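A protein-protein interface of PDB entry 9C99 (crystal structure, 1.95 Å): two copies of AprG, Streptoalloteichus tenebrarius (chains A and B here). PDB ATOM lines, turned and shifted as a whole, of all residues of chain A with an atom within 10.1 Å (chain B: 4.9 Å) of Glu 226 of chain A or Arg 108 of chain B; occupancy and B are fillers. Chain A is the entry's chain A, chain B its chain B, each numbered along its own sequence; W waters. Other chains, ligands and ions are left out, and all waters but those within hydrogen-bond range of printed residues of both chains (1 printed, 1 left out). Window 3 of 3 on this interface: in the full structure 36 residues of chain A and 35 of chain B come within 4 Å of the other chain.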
ATOM      1  N   LEU A 151     -29.903 -10.016 -16.839  1.00  0.00           N
ATOM      2  CA  LEU A 151     -28.589  -9.384 -16.952  1.00  0.00           C
ATOM      3  C   LEU A 151     -28.223  -8.637 -15.674  1.00  0.00           C
ATOM      4  O   LEU A 151     -27.097  -8.750 -15.174  1.00  0.00           O
ATOM      5  CB  LEU A 151     -28.560  -8.416 -18.134  1.00  0.00           C
ATOM      6  CG  LEU A 151     -28.203  -8.976 -19.504  1.00  0.00           C
ATOM      7  CD1 LEU A 151     -28.030  -7.830 -20.502  1.00  0.00           C
ATOM      8  CD2 LEU A 151     -26.945  -9.831 -19.426  1.00  0.00           C
ATOM      9  N   GLY A 154     -27.206 -11.030 -13.020  1.00  0.00           N
ATOM     10  CA  GLY A 154     -26.115 -11.940 -13.291  1.00  0.00           C
ATOM     11  C   GLY A 154     -26.524 -13.302 -13.804  1.00  0.00           C
ATOM     12  O   GLY A 154     -25.677 -14.201 -13.881  1.00  0.00           O
ATOM     13  N   VAL A 156     -26.879 -14.700 -16.704  1.00  0.00           N
ATOM     14  CA  VAL A 156     -26.592 -14.374 -18.097  1.00  0.00           C
ATOM     15  C   VAL A 156     -27.081 -15.477 -19.031  1.00  0.00           C
ATOM     16  O   VAL A 156     -27.502 -15.202 -20.159  1.00  0.00           O
ATOM     17  CB  VAL A 156     -25.088 -14.096 -18.272  1.00  0.00           C
ATOM     18  CG1 VAL A 156     -24.749 -13.845 -19.755  1.00  0.00           C
ATOM     19  CG2 VAL A 156     -24.681 -12.916 -17.426  1.00  0.00           C
ATOM     20  N   ARG A 160     -29.161 -14.997 -22.343  1.00  0.00           N
ATOM     21  CA  ARG A 160     -28.835 -15.509 -23.677  1.00  0.00           C
ATOM     22  C   ARG A 160     -29.998 -16.300 -24.268  1.00  0.00           C
ATOM     23  O   ARG A 160     -30.275 -16.211 -25.470  1.00  0.00           O
ATOM     24  CB  ARG A 160     -27.585 -16.387 -23.614  1.00  0.00           C
ATOM     25  CG  ARG A 160     -26.294 -15.627 -23.378  1.00  0.00           C
ATOM     26  CD  ARG A 160     -25.155 -16.647 -23.446  1.00  0.00           C
ATOM     27  NE  ARG A 160     -23.810 -16.097 -23.314  1.00  0.00           N
ATOM     28  CZ  ARG A 160     -23.063 -15.665 -24.328  1.00  0.00           C
ATOM     29  NH1 ARG A 160     -23.518 -15.691 -25.579  1.00  0.00           N
ATOM     30  NH2 ARG A 160     -21.846 -15.205 -24.085  1.00  0.00           N
ATOM     31  N   LEU A 218     -31.220  -6.526 -26.344  1.00  0.00           N
ATOM     32  CA  LEU A 218     -30.171  -7.222 -27.109  1.00  0.00           C
ATOM     33  C   LEU A 218     -28.894  -6.405 -27.148  1.00  0.00           C
ATOM     34  O   LEU A 218     -27.797  -6.966 -27.105  1.00  0.00           O
ATOM     35  CB  LEU A 218     -30.641  -7.515 -28.530  1.00  0.00           C
ATOM     36  CG  LEU A 218     -31.745  -8.579 -28.626  1.00  0.00           C
ATOM     37  CD1 LEU A 218     -32.504  -8.385 -29.939  1.00  0.00           C
ATOM     38  CD2 LEU A 218     -31.110  -9.971 -28.501  1.00  0.00           C
ATOM     39  N   THR A 219     -29.011  -5.075 -27.160  1.00  0.00           N
ATOM     40  CA  THR A 219     -27.799  -4.260 -27.155  1.00  0.00           C
ATOM     41  C   THR A 219     -27.068  -4.376 -25.825  1.00  0.00           C
ATOM     42  O   THR A 219     -25.842  -4.529 -25.798  1.00  0.00           O
ATOM     43  CB  THR A 219     -28.143  -2.820 -27.483  1.00  0.00           C
ATOM     44  OG1 THR A 219     -28.907  -2.806 -28.690  1.00  0.00           O
ATOM     45  CG2 THR A 219     -26.884  -2.003 -27.692  1.00  0.00           C
ATOM     46  N   ALA A 220     -27.811  -4.349 -24.717  1.00  0.00           N
ATOM     47  CA  ALA A 220     -27.210  -4.547 -23.403  1.00  0.00           C
ATOM     48  C   ALA A 220     -26.598  -5.941 -23.273  1.00  0.00           C
ATOM     49  O   ALA A 220     -25.554  -6.119 -22.628  1.00  0.00           O
ATOM     50  CB  ALA A 220     -28.275  -4.311 -22.326  1.00  0.00           C
ATOM     51  N   LEU A 221     -27.239  -6.945 -23.868  1.00  0.00           N
ATOM     52  CA  LEU A 221     -26.690  -8.288 -23.814  1.00  0.00           C
ATOM     53  C   LEU A 221     -25.407  -8.379 -24.620  1.00  0.00           C
ATOM     54  O   LEU A 221     -24.466  -9.073 -24.216  1.00  0.00           O
ATOM     55  CB  LEU A 221     -27.705  -9.309 -24.334  1.00  0.00           C
ATOM     56  CG  LEU A 221     -27.180 -10.763 -24.379  1.00  0.00           C
ATOM     57  CD1 LEU A 221     -26.814 -11.321 -22.987  1.00  0.00           C
ATOM     58  CD2 LEU A 221     -28.212 -11.634 -25.063  1.00  0.00           C
ATOM     59  N   TYR A 222     -25.345  -7.684 -25.760  1.00  0.00           N
ATOM     60  CA  TYR A 222     -24.074  -7.583 -26.482  1.00  0.00           C
ATOM     61  C   TYR A 222     -22.988  -6.959 -25.609  1.00  0.00           C
ATOM     62  O   TYR A 222     -21.866  -7.470 -25.525  1.00  0.00           O
ATOM     63  CB  TYR A 222     -24.239  -6.767 -27.765  1.00  0.00           C
ATOM     64  CG  TYR A 222     -22.898  -6.438 -28.370  1.00  0.00           C
ATOM     65  CD1 TYR A 222     -22.107  -7.445 -28.906  1.00  0.00           C
ATOM     66  CD2 TYR A 222     -22.393  -5.140 -28.347  1.00  0.00           C
ATOM     67  CE1 TYR A 222     -20.857  -7.172 -29.447  1.00  0.00           C
ATOM     68  CE2 TYR A 222     -21.137  -4.853 -28.879  1.00  0.00           C
ATOM     69  CZ  TYR A 222     -20.380  -5.878 -29.436  1.00  0.00           C
ATOM     70  OH  TYR A 222     -19.137  -5.624 -29.978  1.00  0.00           O
ATOM     71  N   GLU A 223     -23.298  -5.841 -24.956  1.00  0.00           N
ATOM     72  CA  GLU A 223     -22.310  -5.214 -24.084  1.00  0.00           C
ATOM     73  C   GLU A 223     -21.832  -6.177 -22.993  1.00  0.00           C
ATOM     74  O   GLU A 223     -20.638  -6.232 -22.693  1.00  0.00           O
ATOM     75  CB  GLU A 223     -22.891  -3.925 -23.480  1.00  0.00           C
ATOM     76  CG  GLU A 223     -21.958  -3.293 -22.458  1.00  0.00           C
ATOM     77  CD  GLU A 223     -22.242  -1.824 -22.183  1.00  0.00           C
ATOM     78  OE1 GLU A 223     -21.295  -1.110 -21.796  1.00  0.00           O
ATOM     79  OE2 GLU A 223     -23.394  -1.375 -22.348  1.00  0.00           O
ATOM     80  N   ALA A 224     -22.740  -6.982 -22.422  1.00  0.00           N
ATOM     81  CA  ALA A 224     -22.362  -7.926 -21.358  1.00  0.00           C
ATOM     82  C   ALA A 224     -21.469  -9.056 -21.868  1.00  0.00           C
ATOM     83  O   ALA A 224     -20.587  -9.536 -21.138  1.00  0.00           O
ATOM     84  CB  ALA A 224     -23.608  -8.535 -20.716  1.00  0.00           C
ATOM     85  N   THR A 225     -21.716  -9.537 -23.095  1.00  0.00           N
ATOM     86  CA  THR A 225     -21.090 -10.767 -23.583  1.00  0.00           C
ATOM     87  C   THR A 225     -20.085 -10.548 -24.703  1.00  0.00           C
ATOM     88  O   THR A 225     -19.224 -11.409 -24.913  1.00  0.00           O
ATOM     89  CB  THR A 225     -22.135 -11.752 -24.129  1.00  0.00           C
ATOM     90  OG1 THR A 225     -22.773 -11.159 -25.269  1.00  0.00           O
ATOM     91  CG2 THR A 225     -23.173 -12.140 -23.078  1.00  0.00           C
ATOM     92  N   GLU A 226     -20.208  -9.455 -25.448  1.00  0.00           N
ATOM     93  CA  GLU A 226     -19.438  -9.204 -26.660  1.00  0.00           C
ATOM     94  C   GLU A 226     -19.723 -10.240 -27.741  1.00  0.00           C
ATOM     95  O   GLU A 226     -18.934 -10.410 -28.668  1.00  0.00           O
ATOM     96  CB  GLU A 226     -17.936  -9.117 -26.354  1.00  0.00           C
ATOM     97  CG  GLU A 226     -17.495  -7.699 -26.021  1.00  0.00           C
ATOM     98  CD  GLU A 226     -16.256  -7.641 -25.139  1.00  0.00           C
ATOM     99  OE1 GLU A 226     -16.219  -6.746 -24.264  1.00  0.00           O
ATOM    100  OE2 GLU A 226     -15.337  -8.481 -25.311  1.00  0.00           O
ATOM    101  N   ASP A 227     -20.855 -10.939 -27.646  1.00  0.00           N
ATOM    102  CA  ASP A 227     -21.285 -11.837 -28.714  1.00  0.00           C
ATOM    103  C   ASP A 227     -21.988 -11.010 -29.791  1.00  0.00           C
ATOM    104  O   ASP A 227     -23.085 -10.477 -29.579  1.00  0.00           O
ATOM    105  CB  ASP A 227     -22.184 -12.936 -28.146  1.00  0.00           C
ATOM    106  CG  ASP A 227     -22.499 -14.020 -29.160  1.00  0.00           C
ATOM    107  OD1 ASP A 227     -22.435 -13.757 -30.387  1.00  0.00           O
ATOM    108  OD2 ASP A 227     -22.818 -15.139 -28.722  1.00  0.00           O
ATOM    109  N   ARG A 228     -21.360 -10.904 -30.957  1.00  0.00           N
ATOM    110  CA  ARG A 228     -21.891 -10.034 -31.993  1.00  0.00           C
ATOM    111  C   ARG A 228     -23.213 -10.522 -32.580  1.00  0.00           C
ATOM    112  O   ARG A 228     -23.911  -9.713 -33.196  1.00  0.00           O
ATOM    113  CB  ARG A 228     -20.844  -9.857 -33.097  1.00  0.00           C
ATOM    114  CG  ARG A 228     -19.606  -9.087 -32.608  1.00  0.00           C
ATOM    115  CD  ARG A 228     -18.649  -8.758 -33.759  1.00  0.00           C
ATOM    116  NE  ARG A 228     -19.178  -7.743 -34.662  1.00  0.00           N
ATOM    117  CZ  ARG A 228     -18.967  -6.438 -34.520  1.00  0.00           C
ATOM    118  NH1 ARG A 228     -18.238  -5.991 -33.501  1.00  0.00           N
ATOM    119  NH2 ARG A 228     -19.490  -5.581 -35.394  1.00  0.00           N
ATOM    120  N   ALA A 229     -23.575 -11.804 -32.427  1.00  0.00           N
ATOM    121  CA  ALA A 229     -24.912 -12.223 -32.842  1.00  0.00           C
ATOM    122  C   ALA A 229     -25.985 -11.319 -32.237  1.00  0.00           C
ATOM    123  O   ALA A 229     -26.957 -10.969 -32.909  1.00  0.00           O
ATOM    124  CB  ALA A 229     -25.167 -13.684 -32.457  1.00  0.00           C
ATOM    125  N   TYR A 230     -25.816 -10.911 -30.970  1.00  0.00           N
ATOM    126  CA  TYR A 230     -26.800 -10.041 -30.333  1.00  0.00           C
ATOM    127  C   TYR A 230     -26.725  -8.621 -30.872  1.00  0.00           C
ATOM    128  O   TYR A 230     -27.760  -7.955 -31.025  1.00  0.00           O
ATOM    129  CB  TYR A 230     -26.605 -10.025 -28.815  1.00  0.00           C
ATOM    130  CG  TYR A 230     -26.507 -11.399 -28.221  1.00  0.00           C
ATOM    131  CD1 TYR A 230     -27.413 -12.385 -28.579  1.00  0.00           C
ATOM    132  CD2 TYR A 230     -25.483 -11.719 -27.319  1.00  0.00           C
ATOM    133  CE1 TYR A 230     -27.318 -13.668 -28.048  1.00  0.00           C
ATOM    134  CE2 TYR A 230     -25.374 -13.003 -26.774  1.00  0.00           C
ATOM    135  CZ  TYR A 230     -26.304 -13.971 -27.146  1.00  0.00           C
ATOM    136  OH  TYR A 230     -26.221 -15.246 -26.640  1.00  0.00           O
ATOM    137  N   LEU A 231     -25.515  -8.119 -31.125  1.00  0.00           N
ATOM    138  CA  LEU A 231     -25.404  -6.800 -31.747  1.00  0.00           C
ATOM    139  C   LEU A 231     -26.056  -6.794 -33.128  1.00  0.00           C
ATOM    140  O   LEU A 231     -26.759  -5.835 -33.489  1.00  0.00           O
ATOM    141  CB  LEU A 231     -23.938  -6.390 -31.846  1.00  0.00           C
ATOM    142  CG  LEU A 231     -23.656  -5.057 -32.559  1.00  0.00           C
ATOM    143  CD1 LEU A 231     -24.284  -3.907 -31.753  1.00  0.00           C
ATOM    144  CD2 LEU A 231     -22.150  -4.845 -32.700  1.00  0.00           C
ATOM    145  N   ASP A 232     -25.849  -7.873 -33.902  1.00  0.00           N
ATOM    146  CA  ASP A 232     -26.431  -7.986 -35.240  1.00  0.00           C
ATOM    147  C   ASP A 232     -27.951  -7.904 -35.203  1.00  0.00           C
ATOM    148  O   ASP A 232     -28.567  -7.205 -36.013  1.00  0.00           O
ATOM    149  CB  ASP A 232     -26.012  -9.311 -35.892  1.00  0.00           C
ATOM    150  CG  ASP A 232     -24.528  -9.355 -36.268  1.00  0.00           C
ATOM    151  OD1 ASP A 232     -23.865  -8.305 -36.280  1.00  0.00           O
ATOM    152  OD2 ASP A 232     -24.018 -10.461 -36.526  1.00  0.00           O
ATOM    153  N   ARG A 267     -23.212   4.750 -28.282  1.00  0.00           N
ATOM    154  CA  ARG A 267     -22.018   4.619 -27.450  1.00  0.00           C
ATOM    155  C   ARG A 267     -21.175   3.433 -27.913  1.00  0.00           C
ATOM    156  O   ARG A 267     -19.944   3.521 -27.970  1.00  0.00           O
ATOM    157  CB  ARG A 267     -22.385   4.490 -25.960  1.00  0.00           C
ATOM    158  CG  ARG A 267     -21.154   4.364 -25.045  1.00  0.00           C
ATOM    159  CD  ARG A 267     -21.438   4.522 -23.538  1.00  0.00           C
ATOM    160  NE  ARG A 267     -22.369   3.505 -23.043  1.00  0.00           N
ATOM    161  CZ  ARG A 267     -22.067   2.241 -22.755  1.00  0.00           C
ATOM    162  NH1 ARG A 267     -20.833   1.765 -22.901  1.00  0.00           N
ATOM    163  NH2 ARG A 267     -23.020   1.448 -22.310  1.00  0.00           N
ATOM    164  N   LEU A 268     -21.820   2.336 -28.307  1.00  0.00           N
ATOM    165  CA  LEU A 268     -21.052   1.139 -28.640  1.00  0.00           C
ATOM    166  C   LEU A 268     -20.455   1.191 -30.044  1.00  0.00           C
ATOM    167  O   LEU A 268     -19.391   0.621 -30.258  1.00  0.00           O
ATOM    168  CB  LEU A 268     -21.928  -0.116 -28.491  1.00  0.00           C
ATOM    169  CG  LEU A 268     -22.401  -0.367 -27.035  1.00  0.00           C
ATOM    170  CD1 LEU A 268     -23.222  -1.647 -26.882  1.00  0.00           C
ATOM    171  CD2 LEU A 268     -21.209  -0.391 -26.047  1.00  0.00           C
ATOM    172  N   PHE B 104     -22.107  -3.598 -18.320  1.00  0.00           N
ATOM    173  CA  PHE B 104     -21.986  -5.012 -17.996  1.00  0.00           C
ATOM    174  C   PHE B 104     -20.708  -5.623 -18.552  1.00  0.00           C
ATOM    175  O   PHE B 104     -20.231  -6.622 -18.013  1.00  0.00           O
ATOM    176  CB  PHE B 104     -23.197  -5.783 -18.525  1.00  0.00           C
ATOM    177  CG  PHE B 104     -24.498  -5.409 -17.884  1.00  0.00           C
ATOM    178  CD1 PHE B 104     -24.608  -5.313 -16.502  1.00  0.00           C
ATOM    179  CD2 PHE B 104     -25.624  -5.143 -18.670  1.00  0.00           C
ATOM    180  CE1 PHE B 104     -25.799  -4.981 -15.923  1.00  0.00           C
ATOM    181  CE2 PHE B 104     -26.824  -4.801 -18.085  1.00  0.00           C
ATOM    182  CZ  PHE B 104     -26.908  -4.719 -16.715  1.00  0.00           C
ATOM    183  N   GLY B 105     -20.160  -5.081 -19.641  1.00  0.00           N
ATOM    184  CA  GLY B 105     -18.883  -5.586 -20.127  1.00  0.00           C
ATOM    185  C   GLY B 105     -17.743  -5.247 -19.189  1.00  0.00           C
ATOM    186  O   GLY B 105     -16.879  -6.084 -18.908  1.00  0.00           O
ATOM    187  N   LEU B 106     -17.718  -4.010 -18.707  1.00  0.00           N
ATOM    188  CA  LEU B 106     -16.736  -3.617 -17.701  1.00  0.00           C
ATOM    189  C   LEU B 106     -16.859  -4.445 -16.418  1.00  0.00           C
ATOM    190  O   LEU B 106     -15.854  -4.945 -15.901  1.00  0.00           O
ATOM    191  CB  LEU B 106     -16.890  -2.126 -17.415  1.00  0.00           C
ATOM    192  CG  LEU B 106     -16.028  -1.480 -16.343  1.00  0.00           C
ATOM    193  CD1 LEU B 106     -14.560  -1.747 -16.593  1.00  0.00           C
ATOM    194  CD2 LEU B 106     -16.320   0.008 -16.388  1.00  0.00           C
ATOM    195  N   SER B 107     -18.076  -4.593 -15.876  1.00  0.00           N
ATOM    196  CA  SER B 107     -18.214  -5.334 -14.620  1.00  0.00           C
ATOM    197  C   SER B 107     -17.884  -6.804 -14.811  1.00  0.00           C
ATOM    198  O   SER B 107     -17.256  -7.410 -13.940  1.00  0.00           O
ATOM    199  CB  SER B 107     -19.615  -5.155 -14.016  1.00  0.00           C
ATOM    200  OG  SER B 107     -20.613  -5.849 -14.743  1.00  0.00           O
ATOM    201  N   ARG B 108     -18.284  -7.402 -15.948  1.00  0.00           N
ATOM    202  CA  ARG B 108     -17.884  -8.789 -16.194  1.00  0.00           C
ATOM    203  C   ARG B 108     -16.365  -8.925 -16.211  1.00  0.00           C
ATOM    204  O   ARG B 108     -15.812  -9.826 -15.574  1.00  0.00           O
ATOM    205  CB  ARG B 108     -18.468  -9.317 -17.506  1.00  0.00           C
ATOM    206  CG  ARG B 108     -17.937 -10.717 -17.839  1.00  0.00           C
ATOM    207  CD  ARG B 108     -18.425 -11.231 -19.169  1.00  0.00           C
ATOM    208  NE  ARG B 108     -18.008 -10.375 -20.269  1.00  0.00           N
ATOM    209  CZ  ARG B 108     -16.829 -10.469 -20.861  1.00  0.00           C
ATOM    210  NH1 ARG B 108     -15.954 -11.371 -20.441  1.00  0.00           N
ATOM    211  NH2 ARG B 108     -16.529  -9.659 -21.863  1.00  0.00           N
ATOM    212  N   LYS B 109     -15.669  -8.033 -16.914  1.00  0.00           N
ATOM    213  CA  LYS B 109     -14.218  -8.182 -17.008  1.00  0.00           C
ATOM    214  C   LYS B 109     -13.559  -7.953 -15.655  1.00  0.00           C
ATOM    215  O   LYS B 109     -12.648  -8.696 -15.269  1.00  0.00           O
ATOM    216  CB  LYS B 109     -13.647  -7.232 -18.056  1.00  0.00           C
ATOM    217  CG  LYS B 109     -13.921  -7.692 -19.485  1.00  0.00           C
ATOM    218  CD  LYS B 109     -13.768  -6.553 -20.485  1.00  0.00           C
ATOM    219  CE  LYS B 109     -14.199  -7.008 -21.883  1.00  0.00           C
ATOM    220  NZ  LYS B 109     -14.489  -5.866 -22.814  1.00  0.00           N
ATOM    221  N   LEU B 110     -14.052  -6.963 -14.898  1.00  0.00           N
ATOM    222  CA  LEU B 110     -13.473  -6.662 -13.597  1.00  0.00           C
ATOM    223  C   LEU B 110     -13.698  -7.812 -12.630  1.00  0.00           C
ATOM    224  O   LEU B 110     -12.782  -8.222 -11.912  1.00  0.00           O
ATOM    225  CB  LEU B 110     -14.080  -5.368 -13.035  1.00  0.00           C
ATOM    226  CG  LEU B 110     -13.731  -4.037 -13.679  1.00  0.00           C
ATOM    227  CD1 LEU B 110     -14.723  -2.956 -13.183  1.00  0.00           C
ATOM    228  CD2 LEU B 110     -12.299  -3.633 -13.370  1.00  0.00           C
ATOM    229  N   MET B 111     -14.920  -8.343 -12.597  1.00  0.00           N
ATOM    230  CA  MET B 111     -15.236  -9.401 -11.642  1.00  0.00           C
ATOM    231  C   MET B 111     -14.480 -10.689 -11.973  1.00  0.00           C
ATOM    232  O   MET B 111     -14.020 -11.403 -11.076  1.00  0.00           O
ATOM    233  CB  MET B 111     -16.746  -9.640 -11.612  1.00  0.00           C
ATOM    234  CG  MET B 111     -17.215 -10.592 -10.517  1.00  0.00           C
ATOM    235  SD  MET B 111     -17.050  -9.840  -8.880  1.00  0.00           S
ATOM    236  CE  MET B 111     -16.436 -11.228  -7.957  1.00  0.00           C
ATOM    237  N   SER B 112     -14.311 -10.985 -13.257  1.00  0.00           N
ATOM    238  CA  SER B 112     -13.568 -12.180 -13.633  1.00  0.00           C
ATOM    239  C   SER B 112     -12.113 -12.095 -13.191  1.00  0.00           C
ATOM    240  O   SER B 112     -11.536 -13.091 -12.734  1.00  0.00           O
ATOM    241  CB  SER B 112     -13.670 -12.401 -15.140  1.00  0.00           C
ATOM    242  OG  SER B 112     -15.018 -12.743 -15.452  1.00  0.00           O
ATOM    243  N   ARG B 155     -22.774 -13.456  -8.528  1.00  0.00           N
ATOM    244  CA  ARG B 155     -21.907 -14.618  -8.299  1.00  0.00           C
ATOM    245  C   ARG B 155     -22.027 -15.033  -6.830  1.00  0.00           C
ATOM    246  O   ARG B 155     -21.115 -14.893  -6.017  1.00  0.00           O
ATOM    247  CB  ARG B 155     -20.481 -14.292  -8.714  1.00  0.00           C
ATOM    248  CG  ARG B 155     -20.453 -13.665 -10.117  1.00  0.00           C
ATOM    249  CD  ARG B 155     -19.097 -13.622 -10.803  1.00  0.00           C
ATOM    250  NE  ARG B 155     -19.201 -12.875 -12.070  1.00  0.00           N
ATOM    251  CZ  ARG B 155     -18.295 -12.893 -13.054  1.00  0.00           C
ATOM    252  NH1 ARG B 155     -17.189 -13.618 -12.947  1.00  0.00           N
ATOM    253  NH2 ARG B 155     -18.500 -12.178 -14.163  1.00  0.00           N
HETATM  254  O   HOH W   1     -19.483  -2.348 -20.461  1.00  0.00           O
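Among the printed residues, pairs that only touch across the chains: Ala 224 of chain A with Phe 104 of chain B (3.5 Å) and Ala 224 of chain A with Gly 105 of chain B (3.99 Å).
No position is printed for both chains.
Of the 6 pairs that touch across the chains among the printed residues, none has its exchanged pair printed and touching as well.
O of Glu 223 of chain A sits close to N of Gly 105 of chain B, at 3.3 Å.
The backbone carbonyl oxygen (O) of Ala 224 of chain A is in hydrogen-bond range of the guanidinium group (NE) of Arg 108 of chain B, 2.8 Å away.
The side-chain carboxylate (OE1) of Glu 226 of chain A is in salt-bridge range of the side-chain amino group (NZ) of Lys 109 of chain B (2.4 Å).
The guanidinium group of Arg 108 of chain B is in salt-bridge range of the side-chain carboxylate of Glu 226 of chain A.
O of Phe 104 of chain B is in hydrogen-bond range of OG of Ser 107 of chain B, 3.4 Å away.
The guanidinium group of Arg 267 of chain A lies within salt-bridge range of the side-chain carboxylate of Glu 223 of chain A, at 2.8 Å.
O of Arg 108 of chain B is in hydrogen-bond range of OG of Ser 112 of chain B, at 3.0 Å.
Of the printed residues of chain B, Glu 223 of chain A touches Gly 105 (3.2 Å).
Of the printed residues of chain B, Ala 224 of chain A touches Phe 104 (3.5 Å), Gly 105 (3.99 Å) and Arg 108 (2.8 Å).
Glu 226 of chain A touches just these residues of chain B: Arg 108 and Lys 109.
Printed residues of chain A within 4 Å of Phe 104 of chain B: Ala 224.
Of the printed residues of chain A, Gly 105 of chain B touches Glu 223 (3.2 Å) and Ala 224 (3.99 Å).
Ser 107 of chain B touches none of the printed residues of chain A.
Arg 108 of chain B touches just these residues of chain A: Ala 224 and Glu 226.
Of the printed residues of chain A, Lys 109 of chain B touches Glu 226 (2.4 Å).
The nearest printed residue of chain B that does not touch Glu 226 of chain A is Gly 105 of chain B (5.1 Å).
The nearest residue of chain A that does not touch Arg 108 of chain B is Thr 225 of chain A (4.4 Å).
Water W1 lies within hydrogen-bond range of the side-chain carboxylate (OE1) of Glu 223 of chain A (2.6 Å), the backbone NH (N) of Gly 105 of chain B (2.9 Å) and the backbone NH (N) of Leu 106 of chain B (3.0 Å).
Printed residues of chain A that touch a printed residue of chain B: Glu 223, Ala 224 and Glu 226.
Hydrophobic or aromatic side chains of chain A that line the printed part of chain B: Ala 224.
Among the printed residues, Asp or Glu carboxylates within 4 Å of a Lys or Arg side-chain nitrogen of the other chain: Glu 226 of chain A with Arg 108 of chain B (3.8 Å) and Glu 226 of chain A with Lys 109 of chain B (2.4 Å).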
